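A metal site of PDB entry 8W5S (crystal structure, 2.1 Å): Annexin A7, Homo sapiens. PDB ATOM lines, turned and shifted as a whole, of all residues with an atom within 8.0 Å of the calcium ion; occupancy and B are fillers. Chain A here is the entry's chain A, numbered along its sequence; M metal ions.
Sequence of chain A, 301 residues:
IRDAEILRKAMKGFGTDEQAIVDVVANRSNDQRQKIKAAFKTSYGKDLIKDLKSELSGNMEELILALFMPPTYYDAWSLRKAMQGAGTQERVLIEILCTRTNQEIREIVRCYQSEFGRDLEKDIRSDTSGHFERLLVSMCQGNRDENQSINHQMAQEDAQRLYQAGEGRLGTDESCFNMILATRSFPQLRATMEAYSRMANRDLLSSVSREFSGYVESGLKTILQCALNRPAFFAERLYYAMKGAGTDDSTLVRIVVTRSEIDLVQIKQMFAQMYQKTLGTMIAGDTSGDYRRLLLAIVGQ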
ATOM      1  N   ARG A  80      19.755   9.806 -26.924  1.00  0.00           N
ATOM      2  CA  ARG A  80      19.409  11.011 -27.671  1.00  0.00           C
ATOM      3  C   ARG A  80      17.940  11.358 -27.507  1.00  0.00           C
ATOM      4  O   ARG A  80      17.585  12.526 -27.265  1.00  0.00           O
ATOM      5  CB  ARG A  80      19.754  10.838 -29.153  1.00  0.00           C
ATOM      6  CG  ARG A  80      19.551  12.112 -29.976  1.00  0.00           C
ATOM      7  CD  ARG A  80      20.245  13.308 -29.335  1.00  0.00           C
ATOM      8  NE  ARG A  80      19.393  14.492 -29.260  1.00  0.00           N
ATOM      9  CZ  ARG A  80      19.707  15.597 -28.584  1.00  0.00           C
ATOM     10  NH1 ARG A  80      20.847  15.707 -27.935  1.00  0.00           N
ATOM     11  NH2 ARG A  80      18.845  16.609 -28.573  1.00  0.00           N
ATOM     12  N   ALA A  82      16.054  10.632 -25.096  1.00  0.00           N
ATOM     13  CA  ALA A  82      15.759  11.007 -23.718  1.00  0.00           C
ATOM     14  C   ALA A  82      16.156  12.443 -23.410  1.00  0.00           C
ATOM     15  O   ALA A  82      15.700  12.999 -22.405  1.00  0.00           O
ATOM     16  CB  ALA A  82      16.454  10.058 -22.755  1.00  0.00           C
ATOM     17  N   MET A  83      16.987  13.063 -24.249  1.00  0.00           N
ATOM     18  CA  MET A  83      17.409  14.442 -24.066  1.00  0.00           C
ATOM     19  C   MET A  83      16.826  15.382 -25.125  1.00  0.00           C
ATOM     20  O   MET A  83      17.032  16.594 -25.024  1.00  0.00           O
ATOM     21  CB  MET A  83      18.944  14.542 -24.101  1.00  0.00           C
ATOM     22  CG  MET A  83      19.645  14.088 -22.837  1.00  0.00           C
ATOM     23  SD  MET A  83      21.435  14.034 -23.044  1.00  0.00           S
ATOM     24  CE  MET A  83      21.660  12.466 -23.880  1.00  0.00           C
ATOM     25  N   GLN A  84      16.107  14.855 -26.104  1.00  0.00           N
ATOM     26  CA  GLN A  84      15.778  15.610 -27.313  1.00  0.00           C
ATOM     27  C   GLN A  84      14.638  16.593 -27.044  1.00  0.00           C
ATOM     28  O   GLN A  84      13.519  16.187 -26.728  1.00  0.00           O
ATOM     29  CB  GLN A  84      15.420  14.659 -28.446  1.00  0.00           C
ATOM     30  CG  GLN A  84      15.941  15.118 -29.803  1.00  0.00           C
ATOM     31  CD  GLN A  84      15.640  14.126 -30.907  1.00  0.00           C
ATOM     32  OE1 GLN A  84      16.502  13.832 -31.739  1.00  0.00           O
ATOM     33  NE2 GLN A  84      14.421  13.606 -30.921  1.00  0.00           N
ATOM     34  N   GLY A  85      14.930  17.878 -27.197  1.00  0.00           N
ATOM     35  CA  GLY A  85      13.963  18.933 -26.990  1.00  0.00           C
ATOM     36  C   GLY A  85      14.009  19.477 -25.585  1.00  0.00           C
ATOM     37  O   GLY A  85      14.974  19.322 -24.846  1.00  0.00           O
ATOM     38  N   ALA A  86      12.925  20.157 -25.214  1.00  0.00           N
ATOM     39  CA  ALA A  86      12.733  20.488 -23.821  1.00  0.00           C
ATOM     40  C   ALA A  86      12.468  19.223 -23.020  1.00  0.00           C
ATOM     41  O   ALA A  86      12.168  18.157 -23.575  1.00  0.00           O
ATOM     42  CB  ALA A  86      11.586  21.490 -23.655  1.00  0.00           C
ATOM     43  N   GLY A  87      12.603  19.329 -21.704  1.00  0.00           N
ATOM     44  CA  GLY A  87      12.359  18.185 -20.855  1.00  0.00           C
ATOM     45  C   GLY A  87      13.426  17.117 -20.938  1.00  0.00           C
ATOM     46  O   GLY A  87      14.253  17.101 -21.868  1.00  0.00           O
ATOM     47  N   THR A  88      13.426  16.221 -19.957  1.00  0.00           N
ATOM     48  CA  THR A  88      14.385  15.128 -19.861  1.00  0.00           C
ATOM     49  C   THR A  88      13.715  13.978 -19.138  1.00  0.00           C
ATOM     50  O   THR A  88      12.974  14.204 -18.175  1.00  0.00           O
ATOM     51  CB  THR A  88      15.649  15.546 -19.098  1.00  0.00           C
ATOM     52  OG1 THR A  88      16.034  16.877 -19.473  1.00  0.00           O
ATOM     53  CG2 THR A  88      16.792  14.585 -19.378  1.00  0.00           C
ATOM     54  N   ARG A 118      27.180  14.642 -32.364  1.00  0.00           N
ATOM     55  CA  ARG A 118      27.088  15.354 -31.107  1.00  0.00           C
ATOM     56  C   ARG A 118      27.957  14.676 -30.053  1.00  0.00           C
ATOM     57  O   ARG A 118      28.272  13.485 -30.147  1.00  0.00           O
ATOM     58  CB  ARG A 118      25.632  15.439 -30.605  1.00  0.00           C
ATOM     59  CG  ARG A 118      24.797  16.500 -31.300  1.00  0.00           C
ATOM     60  CD  ARG A 118      23.334  16.388 -30.901  1.00  0.00           C
ATOM     61  NE  ARG A 118      23.014  17.208 -29.729  1.00  0.00           N
ATOM     62  CZ  ARG A 118      22.453  18.406 -29.788  1.00  0.00           C
ATOM     63  NH1 ARG A 118      22.141  18.968 -30.946  1.00  0.00           N
ATOM     64  NH2 ARG A 118      22.197  19.052 -28.661  1.00  0.00           N
ATOM     65  N   ASP A 123      25.997  16.828 -24.262  1.00  0.00           N
ATOM     66  CA  ASP A 123      24.540  16.748 -24.217  1.00  0.00           C
ATOM     67  C   ASP A 123      24.040  16.488 -22.796  1.00  0.00           C
ATOM     68  O   ASP A 123      22.975  16.982 -22.414  1.00  0.00           O
ATOM     69  CB  ASP A 123      24.045  15.654 -25.160  1.00  0.00           C
ATOM     70  CG  ASP A 123      23.776  16.177 -26.562  1.00  0.00           C
ATOM     71  OD1 ASP A 123      23.896  17.398 -26.785  1.00  0.00           O
ATOM     72  OD2 ASP A 123      23.447  15.357 -27.456  1.00  0.00           O
ATOM     73  N   SER A 126      24.076  19.693 -20.589  1.00  0.00           N
ATOM     74  CA  SER A 126      23.117  20.727 -20.955  1.00  0.00           C
ATOM     75  C   SER A 126      21.710  20.375 -20.487  1.00  0.00           C
ATOM     76  O   SER A 126      20.952  21.252 -20.062  1.00  0.00           O
ATOM     77  CB  SER A 126      23.145  20.946 -22.466  1.00  0.00           C
ATOM     78  OG  SER A 126      22.142  20.168 -23.106  1.00  0.00           O
ATOM     79  N   ASP A 127      21.344  19.093 -20.556  1.00  0.00           N
ATOM     80  CA  ASP A 127      20.017  18.646 -20.164  1.00  0.00           C
ATOM     81  C   ASP A 127      19.902  18.380 -18.672  1.00  0.00           C
ATOM     82  O   ASP A 127      18.771  18.224 -18.178  1.00  0.00           O
ATOM     83  CB  ASP A 127      19.625  17.382 -20.934  1.00  0.00           C
ATOM     84  CG  ASP A 127      18.370  17.578 -21.744  1.00  0.00           C
ATOM     85  OD1 ASP A 127      18.409  18.349 -22.724  1.00  0.00           O
ATOM     86  OD2 ASP A 127      17.343  16.963 -21.396  1.00  0.00           O
ATOM     87  N   THR A 128      21.007  18.311 -17.949  1.00  0.00           N
ATOM     88  CA  THR A 128      21.011  18.065 -16.523  1.00  0.00           C
ATOM     89  C   THR A 128      21.845  19.138 -15.828  1.00  0.00           C
ATOM     90  O   THR A 128      22.367  20.066 -16.459  1.00  0.00           O
ATOM     91  CB  THR A 128      21.536  16.664 -16.187  1.00  0.00           C
ATOM     92  OG1 THR A 128      22.912  16.559 -16.587  1.00  0.00           O
ATOM     93  CG2 THR A 128      20.713  15.593 -16.901  1.00  0.00           C
HETATM   94 CA    CA M   1      17.100  19.268 -24.191  1.00  0.00          CA
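O of Asp 127 lies within hydrogen-bond range of OG1 of Thr 88 (3.3 Å).
Within 4 Å of the calcium ion: Met 83, Gly 85 and Asp 127.
The calcium ion is bound by OD1 of Asp 127 (2.2 Å), O of Gly 85 (2.2 Å) and O of Met 83 (2.8 Å).
The calcium ion has three donor atoms within binding distance.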
